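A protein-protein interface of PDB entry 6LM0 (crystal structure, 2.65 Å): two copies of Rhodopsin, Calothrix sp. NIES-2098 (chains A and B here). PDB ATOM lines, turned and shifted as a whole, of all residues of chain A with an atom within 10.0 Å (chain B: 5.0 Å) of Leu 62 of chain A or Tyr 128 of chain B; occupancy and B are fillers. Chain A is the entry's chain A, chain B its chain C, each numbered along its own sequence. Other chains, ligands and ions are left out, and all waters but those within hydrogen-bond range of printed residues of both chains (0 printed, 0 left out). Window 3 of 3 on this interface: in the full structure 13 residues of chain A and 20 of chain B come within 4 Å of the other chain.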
ATOM      1  N   THR A   9       0.618 -16.932  30.154  1.00  0.00           N
ATOM      2  CA  THR A   9       0.919 -16.880  28.728  1.00  0.00           C
ATOM      3  C   THR A   9       1.480 -15.519  28.330  1.00  0.00           C
ATOM      4  O   THR A   9       2.528 -15.434  27.678  1.00  0.00           O
ATOM      5  CB  THR A   9      -0.335 -17.204  27.915  1.00  0.00           C
ATOM      6  OG1 THR A   9      -0.724 -18.563  28.156  1.00  0.00           O
ATOM      7  CG2 THR A   9      -0.077 -17.012  26.429  1.00  0.00           C
ATOM      8  N   GLN A  10       0.797 -14.440  28.721  1.00  0.00           N
ATOM      9  CA  GLN A  10       1.266 -13.105  28.361  1.00  0.00           C
ATOM     10  C   GLN A  10       2.571 -12.756  29.063  1.00  0.00           C
ATOM     11  O   GLN A  10       3.390 -12.014  28.509  1.00  0.00           O
ATOM     12  CB  GLN A  10       0.193 -12.064  28.682  1.00  0.00           C
ATOM     13  CG  GLN A  10      -0.957 -12.034  27.686  1.00  0.00           C
ATOM     14  CD  GLN A  10      -0.735 -11.038  26.563  1.00  0.00           C
ATOM     15  OE1 GLN A  10      -0.137  -9.980  26.763  1.00  0.00           O
ATOM     16  NE2 GLN A  10      -1.217 -11.373  25.371  1.00  0.00           N
ATOM     17  N   LEU A  13       5.174 -14.582  27.043  1.00  0.00           N
ATOM     18  CA  LEU A  13       5.294 -13.922  25.747  1.00  0.00           C
ATOM     19  C   LEU A  13       6.141 -12.662  25.863  1.00  0.00           C
ATOM     20  O   LEU A  13       6.903 -12.331  24.946  1.00  0.00           O
ATOM     21  CB  LEU A  13       3.910 -13.592  25.191  1.00  0.00           C
ATOM     22  CG  LEU A  13       3.123 -14.746  24.567  1.00  0.00           C
ATOM     23  CD1 LEU A  13       1.755 -14.266  24.106  1.00  0.00           C
ATOM     24  CD2 LEU A  13       3.896 -15.370  23.415  1.00  0.00           C
ATOM     25  N   TRP A  14       6.027 -11.953  26.989  1.00  0.00           N
ATOM     26  CA  TRP A  14       6.860 -10.778  27.219  1.00  0.00           C
ATOM     27  C   TRP A  14       8.315 -11.170  27.442  1.00  0.00           C
ATOM     28  O   TRP A  14       9.226 -10.499  26.944  1.00  0.00           O
ATOM     29  CB  TRP A  14       6.333  -9.984  28.414  1.00  0.00           C
ATOM     30  CG  TRP A  14       5.303  -8.959  28.049  1.00  0.00           C
ATOM     31  CD1 TRP A  14       3.954  -9.050  28.229  1.00  0.00           C
ATOM     32  CD2 TRP A  14       5.541  -7.682  27.444  1.00  0.00           C
ATOM     33  NE1 TRP A  14       3.336  -7.913  27.772  1.00  0.00           N
ATOM     34  CE2 TRP A  14       4.289  -7.055  27.285  1.00  0.00           C
ATOM     35  CE3 TRP A  14       6.691  -7.008  27.021  1.00  0.00           C
ATOM     36  CZ2 TRP A  14       4.154  -5.789  26.722  1.00  0.00           C
ATOM     37  CZ3 TRP A  14       6.554  -5.751  26.462  1.00  0.00           C
ATOM     38  CH2 TRP A  14       5.296  -5.155  26.317  1.00  0.00           C
ATOM     39  N   PHE A  17       9.759 -11.689  24.166  1.00  0.00           N
ATOM     40  CA  PHE A  17       9.910 -10.440  23.426  1.00  0.00           C
ATOM     41  C   PHE A  17      11.071  -9.612  23.962  1.00  0.00           C
ATOM     42  O   PHE A  17      11.851  -9.051  23.185  1.00  0.00           O
ATOM     43  CB  PHE A  17       8.613  -9.637  23.476  1.00  0.00           C
ATOM     44  CG  PHE A  17       8.730  -8.264  22.879  1.00  0.00           C
ATOM     45  CD1 PHE A  17       8.938  -8.104  21.520  1.00  0.00           C
ATOM     46  CD2 PHE A  17       8.638  -7.136  23.676  1.00  0.00           C
ATOM     47  CE1 PHE A  17       9.049  -6.845  20.964  1.00  0.00           C
ATOM     48  CE2 PHE A  17       8.747  -5.873  23.127  1.00  0.00           C
ATOM     49  CZ  PHE A  17       8.954  -5.727  21.768  1.00  0.00           C
ATOM     50  N   ALA A  54      11.296 -10.761  17.379  1.00  0.00           N
ATOM     51  CA  ALA A  54      10.795  -9.729  18.282  1.00  0.00           C
ATOM     52  C   ALA A  54       9.492  -9.133  17.768  1.00  0.00           C
ATOM     53  O   ALA A  54       8.568  -8.875  18.549  1.00  0.00           O
ATOM     54  CB  ALA A  54      11.846  -8.635  18.470  1.00  0.00           C
ATOM     55  N   ALA A  55       9.399  -8.906  16.458  1.00  0.00           N
ATOM     56  CA  ALA A  55       8.166  -8.377  15.884  1.00  0.00           C
ATOM     57  C   ALA A  55       7.020  -9.365  16.048  1.00  0.00           C
ATOM     58  O   ALA A  55       5.939  -9.005  16.529  1.00  0.00           O
ATOM     59  CB  ALA A  55       8.380  -8.031  14.410  1.00  0.00           C
ATOM     60  N   LEU A  56       7.241 -10.624  15.661  1.00  0.00           N
ATOM     61  CA  LEU A  56       6.182 -11.624  15.754  1.00  0.00           C
ATOM     62  C   LEU A  56       5.772 -11.878  17.198  1.00  0.00           C
ATOM     63  O   LEU A  56       4.602 -12.174  17.466  1.00  0.00           O
ATOM     64  CB  LEU A  56       6.627 -12.927  15.089  1.00  0.00           C
ATOM     65  CG  LEU A  56       6.184 -13.123  13.637  1.00  0.00           C
ATOM     66  CD1 LEU A  56       4.669 -13.055  13.526  1.00  0.00           C
ATOM     67  CD2 LEU A  56       6.839 -12.095  12.724  1.00  0.00           C
ATOM     68  N   TYR A  57       6.713 -11.772  18.139  1.00  0.00           N
ATOM     69  CA  TYR A  57       6.349 -11.884  19.547  1.00  0.00           C
ATOM     70  C   TYR A  57       5.475 -10.718  19.987  1.00  0.00           C
ATOM     71  O   TYR A  57       4.613 -10.885  20.858  1.00  0.00           O
ATOM     72  CB  TYR A  57       7.607 -11.971  20.411  1.00  0.00           C
ATOM     73  CG  TYR A  57       7.926 -13.375  20.868  1.00  0.00           C
ATOM     74  CD1 TYR A  57       7.293 -13.927  21.976  1.00  0.00           C
ATOM     75  CD2 TYR A  57       8.855 -14.154  20.189  1.00  0.00           C
ATOM     76  CE1 TYR A  57       7.580 -15.212  22.397  1.00  0.00           C
ATOM     77  CE2 TYR A  57       9.147 -15.441  20.602  1.00  0.00           C
ATOM     78  CZ  TYR A  57       8.506 -15.964  21.707  1.00  0.00           C
ATOM     79  OH  TYR A  57       8.793 -17.244  22.123  1.00  0.00           O
ATOM     80  N   LEU A  58       5.676  -9.536  19.398  1.00  0.00           N
ATOM     81  CA  LEU A  58       4.785  -8.415  19.674  1.00  0.00           C
ATOM     82  C   LEU A  58       3.408  -8.635  19.061  1.00  0.00           C
ATOM     83  O   LEU A  58       2.404  -8.171  19.613  1.00  0.00           O
ATOM     84  CB  LEU A  58       5.399  -7.113  19.155  1.00  0.00           C
ATOM     85  CG  LEU A  58       4.637  -5.822  19.463  1.00  0.00           C
ATOM     86  CD1 LEU A  58       4.335  -5.715  20.951  1.00  0.00           C
ATOM     87  CD2 LEU A  58       5.420  -4.611  18.985  1.00  0.00           C
ATOM     88  N   THR A  59       3.338  -9.338  17.927  1.00  0.00           N
ATOM     89  CA  THR A  59       2.043  -9.651  17.332  1.00  0.00           C
ATOM     90  C   THR A  59       1.230 -10.576  18.227  1.00  0.00           C
ATOM     91  O   THR A  59      -0.003 -10.475  18.269  1.00  0.00           O
ATOM     92  CB  THR A  59       2.225 -10.284  15.951  1.00  0.00           C
ATOM     93  OG1 THR A  59       2.770 -11.604  16.092  1.00  0.00           O
ATOM     94  CG2 THR A  59       3.153  -9.443  15.089  1.00  0.00           C
ATOM     95  N   MET A  60       1.895 -11.480  18.948  1.00  0.00           N
ATOM     96  CA  MET A  60       1.181 -12.397  19.828  1.00  0.00           C
ATOM     97  C   MET A  60       0.803 -11.730  21.145  1.00  0.00           C
ATOM     98  O   MET A  60      -0.277 -11.993  21.686  1.00  0.00           O
ATOM     99  CB  MET A  60       2.026 -13.645  20.079  1.00  0.00           C
ATOM    100  CG  MET A  60       2.157 -14.541  18.862  1.00  0.00           C
ATOM    101  SD  MET A  60       3.031 -16.072  19.221  1.00  0.00           S
ATOM    102  CE  MET A  60       4.732 -15.524  19.094  1.00  0.00           C
ATOM    103  N   ILE A  61       1.680 -10.871  21.674  1.00  0.00           N
ATOM    104  CA  ILE A  61       1.355 -10.120  22.885  1.00  0.00           C
ATOM    105  C   ILE A  61       0.103  -9.281  22.664  1.00  0.00           C
ATOM    106  O   ILE A  61      -0.817  -9.271  23.491  1.00  0.00           O
ATOM    107  CB  ILE A  61       2.550  -9.249  23.313  1.00  0.00           C
ATOM    108  CG1 ILE A  61       3.680 -10.115  23.869  1.00  0.00           C
ATOM    109  CG2 ILE A  61       2.120  -8.216  24.345  1.00  0.00           C
ATOM    110  CD1 ILE A  61       4.917  -9.324  24.241  1.00  0.00           C
ATOM    111  N   LEU A  62       0.047  -8.570  21.537  1.00  0.00           N
ATOM    112  CA  LEU A  62      -1.120  -7.780  21.172  1.00  0.00           C
ATOM    113  C   LEU A  62      -2.256  -8.626  20.608  1.00  0.00           C
ATOM    114  O   LEU A  62      -3.291  -8.067  20.230  1.00  0.00           O
ATOM    115  CB  LEU A  62      -0.729  -6.703  20.156  1.00  0.00           C
ATOM    116  CG  LEU A  62       0.396  -5.750  20.571  1.00  0.00           C
ATOM    117  CD1 LEU A  62       0.732  -4.788  19.442  1.00  0.00           C
ATOM    118  CD2 LEU A  62       0.024  -4.992  21.835  1.00  0.00           C
ATOM    119  N   GLY A  63      -2.090  -9.945  20.536  1.00  0.00           N
ATOM    120  CA  GLY A  63      -3.154 -10.805  20.055  1.00  0.00           C
ATOM    121  C   GLY A  63      -3.452 -10.685  18.581  1.00  0.00           C
ATOM    122  O   GLY A  63      -4.497 -11.162  18.130  1.00  0.00           O
ATOM    123  N   GLU A  64      -2.557 -10.063  17.810  1.00  0.00           N
ATOM    124  CA  GLU A  64      -2.810  -9.882  16.385  1.00  0.00           C
ATOM    125  C   GLU A  64      -2.665 -11.186  15.610  1.00  0.00           C
ATOM    126  O   GLU A  64      -3.379 -11.398  14.624  1.00  0.00           O
ATOM    127  CB  GLU A  64      -1.868  -8.819  15.817  1.00  0.00           C
ATOM    128  CG  GLU A  64      -1.958  -7.478  16.525  1.00  0.00           C
ATOM    129  CD  GLU A  64      -0.743  -6.606  16.277  1.00  0.00           C
ATOM    130  OE1 GLU A  64       0.314  -7.152  15.897  1.00  0.00           O
ATOM    131  OE2 GLU A  64      -0.846  -5.376  16.463  1.00  0.00           O
ATOM    132  N   THR A  65      -1.759 -12.068  16.034  1.00  0.00           N
ATOM    133  CA  THR A  65      -1.533 -13.341  15.361  1.00  0.00           C
ATOM    134  C   THR A  65      -1.968 -14.527  16.219  1.00  0.00           C
ATOM    135  O   THR A  65      -1.411 -15.622  16.107  1.00  0.00           O
ATOM    136  CB  THR A  65      -0.068 -13.488  14.958  1.00  0.00           C
ATOM    137  OG1 THR A  65       0.775 -13.218  16.086  1.00  0.00           O
ATOM    138  CG2 THR A  65       0.274 -12.531  13.825  1.00  0.00           C
ATOM    139  N   VAL A  66      -2.958 -14.318  17.082  1.00  0.00           N
ATOM    140  CA  VAL A  66      -3.547 -15.376  17.897  1.00  0.00           C
ATOM    141  C   VAL A  66      -5.029 -15.438  17.557  1.00  0.00           C
ATOM    142  O   VAL A  66      -5.746 -14.442  17.704  1.00  0.00           O
ATOM    143  CB  VAL A  66      -3.333 -15.133  19.399  1.00  0.00           C
ATOM    144  CG1 VAL A  66      -3.476 -16.431  20.169  1.00  0.00           C
ATOM    145  CG2 VAL A  66      -1.965 -14.514  19.649  1.00  0.00           C
ATOM    146  N   THR A  67      -5.487 -16.605  17.100  1.00  0.00           N
ATOM    147  CA  THR A  67      -6.829 -16.728  16.556  1.00  0.00           C
ATOM    148  C   THR A  67      -7.409 -18.109  16.829  1.00  0.00           C
ATOM    149  O   THR A  67      -6.712 -19.112  16.609  1.00  0.00           O
ATOM    150  CB  THR A  67      -6.821 -16.462  15.048  1.00  0.00           C
ATOM    151  OG1 THR A  67      -6.433 -15.104  14.802  1.00  0.00           O
ATOM    152  CG2 THR A  67      -8.193 -16.714  14.443  1.00  0.00           C
ATOM    153  N   PHE A  75      -1.761 -19.996  18.099  1.00  0.00           N
ATOM    154  CA  PHE A  75      -0.741 -18.950  18.024  1.00  0.00           C
ATOM    155  C   PHE A  75       0.004 -19.086  16.696  1.00  0.00           C
ATOM    156  O   PHE A  75       1.156 -19.519  16.627  1.00  0.00           O
ATOM    157  CB  PHE A  75       0.213 -19.040  19.210  1.00  0.00           C
ATOM    158  CG  PHE A  75      -0.438 -18.794  20.544  1.00  0.00           C
ATOM    159  CD1 PHE A  75      -0.225 -17.604  21.222  1.00  0.00           C
ATOM    160  CD2 PHE A  75      -1.246 -19.756  21.129  1.00  0.00           C
ATOM    161  CE1 PHE A  75      -0.815 -17.374  22.451  1.00  0.00           C
ATOM    162  CE2 PHE A  75      -1.839 -19.532  22.355  1.00  0.00           C
ATOM    163  CZ  PHE A  75      -1.623 -18.339  23.018  1.00  0.00           C
ATOM    164  N   GLY B 121       0.174  -2.154  11.113  1.00  0.00           N
ATOM    165  CA  GLY B 121      -0.414  -0.915  11.589  1.00  0.00           C
ATOM    166  C   GLY B 121      -1.641  -0.499  10.804  1.00  0.00           C
ATOM    167  O   GLY B 121      -2.563   0.102  11.362  1.00  0.00           O
ATOM    168  N   GLU B 124      -4.756  -2.315  12.331  1.00  0.00           N
ATOM    169  CA  GLU B 124      -4.886  -2.307  13.780  1.00  0.00           C
ATOM    170  C   GLU B 124      -5.682  -1.090  14.246  1.00  0.00           C
ATOM    171  O   GLU B 124      -5.941  -0.149  13.491  1.00  0.00           O
ATOM    172  CB  GLU B 124      -3.497  -2.352  14.437  1.00  0.00           C
ATOM    173  CG  GLU B 124      -3.490  -2.708  15.923  1.00  0.00           C
ATOM    174  CD  GLU B 124      -3.686  -4.190  16.191  1.00  0.00           C
ATOM    175  OE1 GLU B 124      -3.564  -4.998  15.247  1.00  0.00           O
ATOM    176  OE2 GLU B 124      -3.968  -4.548  17.355  1.00  0.00           O
ATOM    177  N   ALA B 125      -6.079  -1.139  15.519  1.00  0.00           N
ATOM    178  CA  ALA B 125      -6.915  -0.132  16.146  1.00  0.00           C
ATOM    179  C   ALA B 125      -6.140   1.171  16.348  1.00  0.00           C
ATOM    180  O   ALA B 125      -4.912   1.196  16.264  1.00  0.00           O
ATOM    181  CB  ALA B 125      -7.444  -0.670  17.478  1.00  0.00           C
ATOM    182  N   PRO B 126      -6.842   2.275  16.615  1.00  0.00           N
ATOM    183  CA  PRO B 126      -6.175   3.579  16.799  1.00  0.00           C
ATOM    184  C   PRO B 126      -5.095   3.574  17.871  1.00  0.00           C
ATOM    185  O   PRO B 126      -4.147   4.368  17.779  1.00  0.00           O
ATOM    186  CB  PRO B 126      -7.334   4.509  17.187  1.00  0.00           C
ATOM    187  CG  PRO B 126      -8.503   3.935  16.484  1.00  0.00           C
ATOM    188  CD  PRO B 126      -8.303   2.436  16.474  1.00  0.00           C
ATOM    189  N   PRO B 127      -5.195   2.755  18.927  1.00  0.00           N
ATOM    190  CA  PRO B 127      -4.062   2.718  19.876  1.00  0.00           C
ATOM    191  C   PRO B 127      -2.773   2.184  19.269  1.00  0.00           C
ATOM    192  O   PRO B 127      -1.720   2.820  19.406  1.00  0.00           O
ATOM    193  CB  PRO B 127      -4.582   1.825  21.016  1.00  0.00           C
ATOM    194  CG  PRO B 127      -5.801   1.160  20.487  1.00  0.00           C
ATOM    195  CD  PRO B 127      -6.389   2.138  19.534  1.00  0.00           C
ATOM    196  N   TYR B 128      -2.823   1.042  18.584  1.00  0.00           N
ATOM    197  CA  TYR B 128      -1.610   0.332  18.200  1.00  0.00           C
ATOM    198  C   TYR B 128      -1.219   0.510  16.737  1.00  0.00           C
ATOM    199  O   TYR B 128      -0.155   0.024  16.337  1.00  0.00           O
ATOM    200  CB  TYR B 128      -1.762  -1.161  18.513  1.00  0.00           C
ATOM    201  CG  TYR B 128      -2.055  -1.428  19.970  1.00  0.00           C
ATOM    202  CD1 TYR B 128      -1.032  -1.459  20.907  1.00  0.00           C
ATOM    203  CD2 TYR B 128      -3.357  -1.631  20.411  1.00  0.00           C
ATOM    204  CE1 TYR B 128      -1.293  -1.695  22.242  1.00  0.00           C
ATOM    205  CE2 TYR B 128      -3.628  -1.869  21.746  1.00  0.00           C
ATOM    206  CZ  TYR B 128      -2.591  -1.900  22.656  1.00  0.00           C
ATOM    207  OH  TYR B 128      -2.848  -2.135  23.988  1.00  0.00           O
ATOM    208  N   ASN B 129      -2.039   1.186  15.929  1.00  0.00           N
ATOM    209  CA  ASN B 129      -1.608   1.501  14.571  1.00  0.00           C
ATOM    210  C   ASN B 129      -0.450   2.492  14.576  1.00  0.00           C
ATOM    211  O   ASN B 129       0.404   2.454  13.682  1.00  0.00           O
ATOM    212  CB  ASN B 129      -2.782   2.048  13.755  1.00  0.00           C
ATOM    213  CG  ASN B 129      -3.356   3.320  14.337  1.00  0.00           C
ATOM    214  OD1 ASN B 129      -3.059   3.682  15.473  1.00  0.00           O
ATOM    215  ND2 ASN B 129      -4.179   4.008  13.559  1.00  0.00           N
ATOM    216  N   TYR B 130      -0.398   3.375  15.577  1.00  0.00           N
ATOM    217  CA  TYR B 130       0.728   4.295  15.698  1.00  0.00           C
ATOM    218  C   TYR B 130       1.978   3.571  16.183  1.00  0.00           C
ATOM    219  O   TYR B 130       3.092   3.893  15.754  1.00  0.00           O
ATOM    220  CB  TYR B 130       0.374   5.440  16.646  1.00  0.00           C
ATOM    221  CG  TYR B 130      -0.887   6.184  16.271  1.00  0.00           C
ATOM    222  CD1 TYR B 130      -1.084   6.647  14.977  1.00  0.00           C
ATOM    223  CD2 TYR B 130      -1.881   6.423  17.210  1.00  0.00           C
ATOM    224  CE1 TYR B 130      -2.236   7.328  14.629  1.00  0.00           C
ATOM    225  CE2 TYR B 130      -3.037   7.103  16.871  1.00  0.00           C
ATOM    226  CZ  TYR B 130      -3.210   7.552  15.578  1.00  0.00           C
ATOM    227  OH  TYR B 130      -4.357   8.227  15.235  1.00  0.00           O
ATOM    228  N   LEU B 131       1.812   2.594  17.077  1.00  0.00           N
ATOM    229  CA  LEU B 131       2.958   1.848  17.588  1.00  0.00           C
ATOM    230  C   LEU B 131       3.687   1.126  16.462  1.00  0.00           C
ATOM    231  O   LEU B 131       4.921   1.151  16.386  1.00  0.00           O
ATOM    232  CB  LEU B 131       2.500   0.858  18.660  1.00  0.00           C
ATOM    233  CG  LEU B 131       3.459  -0.292  18.972  1.00  0.00           C
ATOM    234  CD1 LEU B 131       4.649   0.205  19.781  1.00  0.00           C
ATOM    235  CD2 LEU B 131       2.734  -1.408  19.706  1.00  0.00           C
ATOM    236  N   TRP B 132       2.935   0.478  15.570  1.00  0.00           N
ATOM    237  CA  TRP B 132       3.556  -0.178  14.425  1.00  0.00           C
ATOM    238  C   TRP B 132       4.066   0.836  13.409  1.00  0.00           C
ATOM    239  O   TRP B 132       5.022   0.550  12.678  1.00  0.00           O
ATOM    240  CB  TRP B 132       2.567  -1.146  13.775  1.00  0.00           C
ATOM    241  CG  TRP B 132       2.352  -2.397  14.574  1.00  0.00           C
ATOM    242  CD1 TRP B 132       1.229  -2.747  15.264  1.00  0.00           C
ATOM    243  CD2 TRP B 132       3.291  -3.463  14.769  1.00  0.00           C
ATOM    244  NE1 TRP B 132       1.408  -3.964  15.876  1.00  0.00           N
ATOM    245  CE2 TRP B 132       2.666  -4.425  15.588  1.00  0.00           C
ATOM    246  CE3 TRP B 132       4.598  -3.698  14.331  1.00  0.00           C
ATOM    247  CZ2 TRP B 132       3.301  -5.603  15.976  1.00  0.00           C
ATOM    248  CZ3 TRP B 132       5.228  -4.868  14.719  1.00  0.00           C
ATOM    249  CH2 TRP B 132       4.580  -5.805  15.533  1.00  0.00           C
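The side-chain carboxylate (OE2) of Glu 64 of chain A lies close to the side-chain carboxylate (OE1) of Glu 124 of chain B (3.0 Å). The side-chain carboxylate (OE2) of Glu 64 of chain A sits at hydrogen-bond distance from the indole nitrogen (NE1) of Trp 132 of chain B (2.7 Å).
Of the 20 printed residues of chain A, 5 touch a printed residue of chain B. Printed residues of chain A that touch a printed residue of chain B: Ala 55, Leu 58, Thr 59, Leu 62 and Glu 64. Among the printed residues, no Asp or Glu carboxylate lies within 4 Å of a Lys or Arg side-chain nitrogen of the other chain.
O of Ala 55 of chain A touches CH2 of Trp 132 of chain B, at 3.6 Å. CG of Leu 58 of chain A touches CZ2 of Trp 132 of chain B, at 3.7 Å. Trp 132 of chain B touches Thr 59 of chain A. Tyr 128 of chain B touches Leu 62 of chain A. Leu 62 of chain A touches Leu 131 of chain B (CD1 to CD2, 3.9 Å). NE1 of Trp 132 of chain B touches CD1 of Leu 62 of chain A, 3.7 Å away.
Of chain B, only Tyr 128 (3.6 Å), Leu 131 (3.9 Å) and Trp 132 (3.7 Å) come within 4 Å of Leu 62 of chain A. Tyr 128 of chain B touches just one residue of chain A: Leu 62 (3.6 Å). No residue of chain A comes within 4 Å of Ala 125 of chain B. No residue of chain A comes within 4 Å of Asn 129 of chain B. Of the printed residues of chain B, Ala 55 of chain A touches Trp 132. Printed residues of chain A within 4 Å of Trp 132 of chain B: Ala 55, Leu 58, Thr 59, Leu 62 and Glu 64. Of the printed residues of chain B, Glu 64 of chain A touches Glu 124 and Trp 132. Of the printed residues of chain B, Leu 58 of chain A touches Trp 132. Ile 61 of chain A touches none of the printed residues of chain B. Tyr 57 of chain A touches none of the printed residues of chain B. The nearest residue of chain B that does not touch Leu 62 of chain A is Glu 124 of chain B (4.6 Å). The nearest residue of chain A that does not touch Tyr 128 of chain B is Glu 64 of chain A (4.8 Å).
No position is printed for both chains.
OG1 of Thr 59 of chain A sits at hydrogen-bond distance from OG1 of Thr 65 of chain A (2.6 Å). N of Glu 64 of chain A is in hydrogen-bond range of O of Thr 59 of chain A.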
